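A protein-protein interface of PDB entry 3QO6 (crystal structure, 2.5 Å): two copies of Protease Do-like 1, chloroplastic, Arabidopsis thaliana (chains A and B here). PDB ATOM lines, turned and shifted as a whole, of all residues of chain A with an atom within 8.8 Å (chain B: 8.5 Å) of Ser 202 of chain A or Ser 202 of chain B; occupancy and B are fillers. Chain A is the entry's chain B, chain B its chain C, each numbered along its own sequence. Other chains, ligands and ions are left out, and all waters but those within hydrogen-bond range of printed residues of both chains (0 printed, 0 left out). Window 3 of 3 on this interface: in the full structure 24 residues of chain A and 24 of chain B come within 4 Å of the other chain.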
ATOM      1  N   PHE A 138     -30.187   3.602  11.103  1.00  0.00           N
ATOM      2  CA  PHE A 138     -30.182   4.996  10.669  1.00  0.00           C
ATOM      3  C   PHE A 138     -31.356   5.347   9.762  1.00  0.00           C
ATOM      4  O   PHE A 138     -31.239   6.244   8.929  1.00  0.00           O
ATOM      5  CB  PHE A 138     -28.878   5.296   9.923  1.00  0.00           C
ATOM      6  CG  PHE A 138     -27.651   4.879  10.677  1.00  0.00           C
ATOM      7  CD1 PHE A 138     -26.699   4.051  10.085  1.00  0.00           C
ATOM      8  CD2 PHE A 138     -27.467   5.276  11.995  1.00  0.00           C
ATOM      9  CE1 PHE A 138     -25.574   3.615  10.797  1.00  0.00           C
ATOM     10  CE2 PHE A 138     -26.341   4.848  12.723  1.00  0.00           C
ATOM     11  CZ  PHE A 138     -25.396   4.015  12.114  1.00  0.00           C
ATOM     12  N   ASN A 176     -26.410  -2.030  13.116  1.00  0.00           N
ATOM     13  CA  ASN A 176     -26.366  -0.689  13.733  1.00  0.00           C
ATOM     14  C   ASN A 176     -27.679  -0.274  14.407  1.00  0.00           C
ATOM     15  O   ASN A 176     -28.671  -0.995  14.344  1.00  0.00           O
ATOM     16  CB  ASN A 176     -26.058   0.394  12.696  1.00  0.00           C
ATOM     17  CG  ASN A 176     -24.718   0.241  12.073  1.00  0.00           C
ATOM     18  OD1 ASN A 176     -24.601  -0.265  10.956  1.00  0.00           O
ATOM     19  ND2 ASN A 176     -23.690   0.677  12.777  1.00  0.00           N
ATOM     20  N   PRO A 177     -27.689   0.895  15.077  1.00  0.00           N
ATOM     21  CA  PRO A 177     -28.914   1.382  15.736  1.00  0.00           C
ATOM     22  C   PRO A 177     -30.025   1.454  14.696  1.00  0.00           C
ATOM     23  O   PRO A 177     -29.867   2.071  13.653  1.00  0.00           O
ATOM     24  CB  PRO A 177     -28.494   2.738  16.252  1.00  0.00           C
ATOM     25  CG  PRO A 177     -27.086   2.434  16.741  1.00  0.00           C
ATOM     26  CD  PRO A 177     -26.498   1.578  15.619  1.00  0.00           C
ATOM     27  N   ILE A 198     -25.294  -4.990  20.142  1.00  0.00           N
ATOM     28  CA  ILE A 198     -23.919  -5.110  19.682  1.00  0.00           C
ATOM     29  C   ILE A 198     -22.924  -4.714  20.784  1.00  0.00           C
ATOM     30  O   ILE A 198     -23.300  -4.164  21.812  1.00  0.00           O
ATOM     31  CB  ILE A 198     -23.698  -4.178  18.506  1.00  0.00           C
ATOM     32  CG1 ILE A 198     -23.711  -2.748  19.024  1.00  0.00           C
ATOM     33  CG2 ILE A 198     -24.804  -4.362  17.440  1.00  0.00           C
ATOM     34  CD1 ILE A 198     -23.504  -1.736  17.940  1.00  0.00           C
ATOM     35  N   TYR A 199     -21.656  -5.030  20.562  1.00  0.00           N
ATOM     36  CA  TYR A 199     -20.571  -4.639  21.458  1.00  0.00           C
ATOM     37  C   TYR A 199     -19.805  -3.635  20.587  1.00  0.00           C
ATOM     38  O   TYR A 199     -19.361  -3.979  19.492  1.00  0.00           O
ATOM     39  CB  TYR A 199     -19.663  -5.817  21.807  1.00  0.00           C
ATOM     40  CG  TYR A 199     -20.086  -6.618  23.024  1.00  0.00           C
ATOM     41  CD1 TYR A 199     -21.199  -6.252  23.794  1.00  0.00           C
ATOM     42  CD2 TYR A 199     -19.378  -7.752  23.408  1.00  0.00           C
ATOM     43  CE1 TYR A 199     -21.587  -7.004  24.914  1.00  0.00           C
ATOM     44  CE2 TYR A 199     -19.755  -8.511  24.517  1.00  0.00           C
ATOM     45  CZ  TYR A 199     -20.851  -8.138  25.268  1.00  0.00           C
ATOM     46  OH  TYR A 199     -21.188  -8.890  26.382  1.00  0.00           O
ATOM     47  N   SER A 200     -19.689  -2.392  21.045  1.00  0.00           N
ATOM     48  CA  SER A 200     -18.997  -1.365  20.274  1.00  0.00           C
ATOM     49  C   SER A 200     -18.725  -0.103  21.089  1.00  0.00           C
ATOM     50  O   SER A 200     -19.630   0.549  21.586  1.00  0.00           O
ATOM     51  CB  SER A 200     -19.818  -0.971  19.034  1.00  0.00           C
ATOM     52  OG  SER A 200     -19.205   0.105  18.344  1.00  0.00           O
ATOM     53  N   PRO A 201     -17.460   0.274  21.207  1.00  0.00           N
ATOM     54  CA  PRO A 201     -17.131   1.481  21.971  1.00  0.00           C
ATOM     55  C   PRO A 201     -17.653   2.750  21.310  1.00  0.00           C
ATOM     56  O   PRO A 201     -17.674   3.802  21.934  1.00  0.00           O
ATOM     57  CB  PRO A 201     -15.623   1.460  22.001  1.00  0.00           C
ATOM     58  CG  PRO A 201     -15.293   0.828  20.670  1.00  0.00           C
ATOM     59  CD  PRO A 201     -16.269  -0.310  20.574  1.00  0.00           C
ATOM     60  N   SER A 202     -18.086   2.653  20.057  1.00  0.00           N
ATOM     61  CA  SER A 202     -18.568   3.834  19.355  1.00  0.00           C
ATOM     62  C   SER A 202     -20.083   3.923  19.210  1.00  0.00           C
ATOM     63  O   SER A 202     -20.633   5.013  19.041  1.00  0.00           O
ATOM     64  CB  SER A 202     -17.925   3.916  17.957  1.00  0.00           C
ATOM     65  OG  SER A 202     -18.439   2.944  17.050  1.00  0.00           O
ATOM     66  N   GLY A 203     -20.760   2.781  19.277  1.00  0.00           N
ATOM     67  CA  GLY A 203     -22.200   2.785  19.101  1.00  0.00           C
ATOM     68  C   GLY A 203     -22.462   2.499  17.638  1.00  0.00           C
ATOM     69  O   GLY A 203     -23.587   2.471  17.165  1.00  0.00           O
ATOM     70  N   ALA A 204     -21.393   2.302  16.900  1.00  0.00           N
ATOM     71  CA  ALA A 204     -21.519   1.993  15.504  1.00  0.00           C
ATOM     72  C   ALA A 204     -21.162   0.512  15.405  1.00  0.00           C
ATOM     73  O   ALA A 204     -20.505  -0.030  16.304  1.00  0.00           O
ATOM     74  CB  ALA A 204     -20.518   2.823  14.710  1.00  0.00           C
ATOM     75  N   SER A 205     -21.585  -0.145  14.327  1.00  0.00           N
ATOM     76  CA  SER A 205     -21.250  -1.541  14.156  1.00  0.00           C
ATOM     77  C   SER A 205     -19.722  -1.732  14.161  1.00  0.00           C
ATOM     78  O   SER A 205     -18.991  -1.051  13.474  1.00  0.00           O
ATOM     79  CB  SER A 205     -21.821  -2.091  12.852  1.00  0.00           C
ATOM     80  OG  SER A 205     -21.563  -3.475  12.796  1.00  0.00           O
ATOM     81  N   SER A 206     -19.259  -2.681  14.948  1.00  0.00           N
ATOM     82  CA  SER A 206     -17.858  -2.964  15.047  1.00  0.00           C
ATOM     83  C   SER A 206     -17.647  -4.457  14.693  1.00  0.00           C
ATOM     84  O   SER A 206     -16.609  -5.064  14.995  1.00  0.00           O
ATOM     85  CB  SER A 206     -17.402  -2.636  16.467  1.00  0.00           C
ATOM     86  OG  SER A 206     -16.044  -2.940  16.684  1.00  0.00           O
ATOM     87  N   GLY A 207     -18.627  -5.040  14.016  1.00  0.00           N
ATOM     88  CA  GLY A 207     -18.494  -6.435  13.669  1.00  0.00           C
ATOM     89  C   GLY A 207     -18.815  -7.487  14.723  1.00  0.00           C
ATOM     90  O   GLY A 207     -18.569  -8.671  14.486  1.00  0.00           O
ATOM     91  N   PHE B 138     -13.261  -8.877  22.825  1.00  0.00           N
ATOM     92  CA  PHE B 138     -14.116  -8.576  23.971  1.00  0.00           C
ATOM     93  C   PHE B 138     -14.419  -9.830  24.781  1.00  0.00           C
ATOM     94  O   PHE B 138     -15.527  -9.984  25.281  1.00  0.00           O
ATOM     95  CB  PHE B 138     -15.459  -7.989  23.534  1.00  0.00           C
ATOM     96  CG  PHE B 138     -15.358  -6.919  22.493  1.00  0.00           C
ATOM     97  CD1 PHE B 138     -16.041  -7.049  21.284  1.00  0.00           C
ATOM     98  CD2 PHE B 138     -14.628  -5.765  22.727  1.00  0.00           C
ATOM     99  CE1 PHE B 138     -16.009  -6.045  20.314  1.00  0.00           C
ATOM    100  CE2 PHE B 138     -14.585  -4.744  21.764  1.00  0.00           C
ATOM    101  CZ  PHE B 138     -15.287  -4.894  20.547  1.00  0.00           C
ATOM    102  N   ASN B 176     -11.043  -6.874  16.564  1.00  0.00           N
ATOM    103  CA  ASN B 176     -11.285  -6.007  17.725  1.00  0.00           C
ATOM    104  C   ASN B 176     -10.378  -6.332  18.913  1.00  0.00           C
ATOM    105  O   ASN B 176      -9.656  -7.327  18.903  1.00  0.00           O
ATOM    106  CB  ASN B 176     -12.748  -6.155  18.220  1.00  0.00           C
ATOM    107  CG  ASN B 176     -13.773  -5.639  17.221  1.00  0.00           C
ATOM    108  OD1 ASN B 176     -14.375  -6.408  16.462  1.00  0.00           O
ATOM    109  ND2 ASN B 176     -13.981  -4.333  17.221  1.00  0.00           N
ATOM    110  N   PRO B 177     -10.377  -5.459  19.938  1.00  0.00           N
ATOM    111  CA  PRO B 177      -9.547  -5.734  21.120  1.00  0.00           C
ATOM    112  C   PRO B 177      -9.903  -7.133  21.572  1.00  0.00           C
ATOM    113  O   PRO B 177     -11.082  -7.469  21.692  1.00  0.00           O
ATOM    114  CB  PRO B 177     -10.008  -4.674  22.089  1.00  0.00           C
ATOM    115  CG  PRO B 177     -10.105  -3.454  21.152  1.00  0.00           C
ATOM    116  CD  PRO B 177     -10.692  -4.015  19.848  1.00  0.00           C
ATOM    117  N   ILE B 198      -5.146  -2.653  14.319  1.00  0.00           N
ATOM    118  CA  ILE B 198      -6.174  -2.103  13.437  1.00  0.00           C
ATOM    119  C   ILE B 198      -6.044  -0.596  13.411  1.00  0.00           C
ATOM    120  O   ILE B 198      -5.470  -0.024  14.321  1.00  0.00           O
ATOM    121  CB  ILE B 198      -7.588  -2.369  14.001  1.00  0.00           C
ATOM    122  CG1 ILE B 198      -7.765  -1.538  15.280  1.00  0.00           C
ATOM    123  CG2 ILE B 198      -7.784  -3.843  14.342  1.00  0.00           C
ATOM    124  CD1 ILE B 198      -9.164  -1.513  15.784  1.00  0.00           C
ATOM    125  N   TYR B 199      -6.580   0.041  12.375  1.00  0.00           N
ATOM    126  CA  TYR B 199      -6.605   1.512  12.299  1.00  0.00           C
ATOM    127  C   TYR B 199      -8.042   1.905  12.621  1.00  0.00           C
ATOM    128  O   TYR B 199      -8.945   1.543  11.880  1.00  0.00           O
ATOM    129  CB  TYR B 199      -6.343   2.061  10.893  1.00  0.00           C
ATOM    130  CG  TYR B 199      -4.915   2.309  10.526  1.00  0.00           C
ATOM    131  CD1 TYR B 199      -3.931   2.433  11.500  1.00  0.00           C
ATOM    132  CD2 TYR B 199      -4.526   2.379   9.181  1.00  0.00           C
ATOM    133  CE1 TYR B 199      -2.566   2.607  11.140  1.00  0.00           C
ATOM    134  CE2 TYR B 199      -3.186   2.555   8.812  1.00  0.00           C
ATOM    135  CZ  TYR B 199      -2.210   2.660   9.792  1.00  0.00           C
ATOM    136  OH  TYR B 199      -0.878   2.749   9.439  1.00  0.00           O
ATOM    137  N   SER B 200      -8.279   2.629  13.705  1.00  0.00           N
ATOM    138  CA  SER B 200      -9.652   3.034  13.982  1.00  0.00           C
ATOM    139  C   SER B 200      -9.776   4.221  14.885  1.00  0.00           C
ATOM    140  O   SER B 200      -9.145   4.297  15.912  1.00  0.00           O
ATOM    141  CB  SER B 200     -10.457   1.887  14.599  1.00  0.00           C
ATOM    142  OG  SER B 200     -11.853   2.178  14.609  1.00  0.00           O
ATOM    143  N   PRO B 201     -10.613   5.173  14.508  1.00  0.00           N
ATOM    144  CA  PRO B 201     -10.832   6.374  15.315  1.00  0.00           C
ATOM    145  C   PRO B 201     -11.453   5.970  16.657  1.00  0.00           C
ATOM    146  O   PRO B 201     -11.171   6.559  17.705  1.00  0.00           O
ATOM    147  CB  PRO B 201     -11.832   7.164  14.476  1.00  0.00           C
ATOM    148  CG  PRO B 201     -11.492   6.763  13.081  1.00  0.00           C
ATOM    149  CD  PRO B 201     -11.320   5.274  13.224  1.00  0.00           C
ATOM    150  N   SER B 202     -12.281   4.931  16.597  1.00  0.00           N
ATOM    151  CA  SER B 202     -13.041   4.429  17.734  1.00  0.00           C
ATOM    152  C   SER B 202     -12.364   3.415  18.626  1.00  0.00           C
ATOM    153  O   SER B 202     -12.825   3.156  19.740  1.00  0.00           O
ATOM    154  CB  SER B 202     -14.351   3.803  17.223  1.00  0.00           C
ATOM    155  OG  SER B 202     -14.126   2.608  16.469  1.00  0.00           O
ATOM    156  N   GLY B 203     -11.285   2.818  18.151  1.00  0.00           N
ATOM    157  CA  GLY B 203     -10.665   1.793  18.962  1.00  0.00           C
ATOM    158  C   GLY B 203     -11.388   0.481  18.692  1.00  0.00           C
ATOM    159  O   GLY B 203     -11.150  -0.516  19.352  1.00  0.00           O
ATOM    160  N   ALA B 204     -12.292   0.481  17.722  1.00  0.00           N
ATOM    161  CA  ALA B 204     -12.996  -0.738  17.382  1.00  0.00           C
ATOM    162  C   ALA B 204     -12.957  -0.960  15.860  1.00  0.00           C
ATOM    163  O   ALA B 204     -12.795  -0.009  15.087  1.00  0.00           O
ATOM    164  CB  ALA B 204     -14.386  -0.662  17.859  1.00  0.00           C
ATOM    165  N   SER B 205     -13.118  -2.211  15.442  1.00  0.00           N
ATOM    166  CA  SER B 205     -13.049  -2.548  14.031  1.00  0.00           C
ATOM    167  C   SER B 205     -13.767  -1.590  13.118  1.00  0.00           C
ATOM    168  O   SER B 205     -14.957  -1.292  13.291  1.00  0.00           O
ATOM    169  CB  SER B 205     -13.563  -3.961  13.756  1.00  0.00           C
ATOM    170  OG  SER B 205     -13.541  -4.227  12.351  1.00  0.00           O
ATOM    171  N   SER B 206     -13.039  -1.136  12.112  1.00  0.00           N
ATOM    172  CA  SER B 206     -13.593  -0.201  11.172  1.00  0.00           C
ATOM    173  C   SER B 206     -13.265  -0.756   9.795  1.00  0.00           C
ATOM    174  O   SER B 206     -13.266  -0.051   8.781  1.00  0.00           O
ATOM    175  CB  SER B 206     -12.967   1.181  11.414  1.00  0.00           C
ATOM    176  OG  SER B 206     -13.538   2.181  10.585  1.00  0.00           O
ATOM    177  N   GLY B 207     -12.978  -2.046   9.761  1.00  0.00           N
ATOM    178  CA  GLY B 207     -12.653  -2.657   8.485  1.00  0.00           C
ATOM    179  C   GLY B 207     -11.208  -2.552   8.009  1.00  0.00           C
ATOM    180  O   GLY B 207     -10.905  -2.895   6.861  1.00  0.00           O
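Among the printed residues, pairs that only touch across the chains: Ser 206 of chain A with Ala 204 of chain B (3.1 Å), Pro 201 of chain A with Ala 204 of chain B (3.3 Å), Pro 201 of chain A with Ser 202 of chain B (3.5 Å), Ser 202 of chain A with Ser 202 of chain B (3.7 Å) and Tyr 199 of chain A with Phe 138 of chain B (3.9 Å).
N of Phe 138 of chain B sits at hydrogen-bond distance from O of Pro 177 of chain B (2.8 Å).
N of Ser 205 of chain B sits close to ND2 of Asn 176 of chain B, 2.9 Å away.
The side-chain hydroxyl (OG) of Ser 200 of chain A sits at hydrogen-bond distance from the side-chain hydroxyl (OG) of Ser 202 of chain A (3.2 Å).
OG of Ser 202 of chain A is in hydrogen-bond range of N of Ala 204 of chain A (3.0 Å).
OG of Ser 200 of chain B lies within hydrogen-bond range of OG of Ser 202 of chain B (3.0 Å).
The side-chain hydroxyl (OG) of Ser 202 of chain B lies close to the backbone NH (N) of Ala 204 of chain B, 3.1 Å away.
ND2 of Asn 176 of chain B lies within hydrogen-bond range of OG of Ser 206 of chain A, at 2.5 Å.
N of Ser 205 of chain B lies within hydrogen-bond range of OG of Ser 206 of chain A (3.3 Å).
Pro 201 of chain A touches Ser 202 of chain B, but with the chains exchanged Ser 202 of chain A does not touch Pro 201 of chain B (6.9 Å).
Ser 202 of chain B touches its own counterpart, Ser 202 of chain A.
Ser 206 of chain A touches Asn 176 of chain B, but with the chains exchanged Asn 176 of chain A does not touch Ser 206 of chain B (10.3 Å).
Ser 206 of chain A touches Ser 205 of chain B, but with the chains exchanged Ser 205 of chain A does not touch Ser 206 of chain B (5.9 Å).
Of the 13 printed residues of chain A, 4 touch a printed residue of chain B.
Hydrophobic or aromatic side chains of chain A that line the printed part of chain B: Tyr 199 and Pro 201.
Hydrophobic or aromatic side chains of chain B within 4 Å of the printed part of chain A: Phe 138 and Ala 204.
Among the printed residues, no Asp or Glu carboxylate lies within 4 Å of a Lys or Arg side-chain nitrogen of the other chain.
Ser 202 of chain A touches just one residue of chain B: Ser 202.
Of chain A, only Pro 201 (3.5 Å) and Ser 202 (3.7 Å) come within 4 Å of Ser 202 of chain B.
Pro 201 of chain A touches just these residues of chain B: Ser 202 (3.5 Å) and Ala 204 (3.3 Å).
No residue of chain B comes within 4 Å of Ala 204 of chain A.
No residue of chain A comes within 4 Å of Pro 201 of chain B.
No residue of chain A comes within 4 Å of Gly 203 of chain B.
Of chain A, only Pro 201 and Ser 206 come within 4 Å of Ala 204 of chain B.
Of the printed residues of chain A, Asn 176 of chain B touches Ser 206 (2.5 Å).
Of the printed residues of chain B, Ser 206 of chain A touches Asn 176 (2.5 Å), Ala 204 (3.1 Å) and Ser 205 (3.3 Å).
Of the printed residues of chain A, Phe 138 of chain B touches Tyr 199 (3.9 Å).
Printed residues of chain A within 4 Å of Ser 205 of chain B: Ser 206 (3.3 Å).
The nearest residue of chain B that does not touch Ser 202 of chain A is Ala 204 of chain B (5.4 Å).
The nearest residue of chain A that does not touch Ser 202 of chain B is Ser 206 of chain A (5.9 Å).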
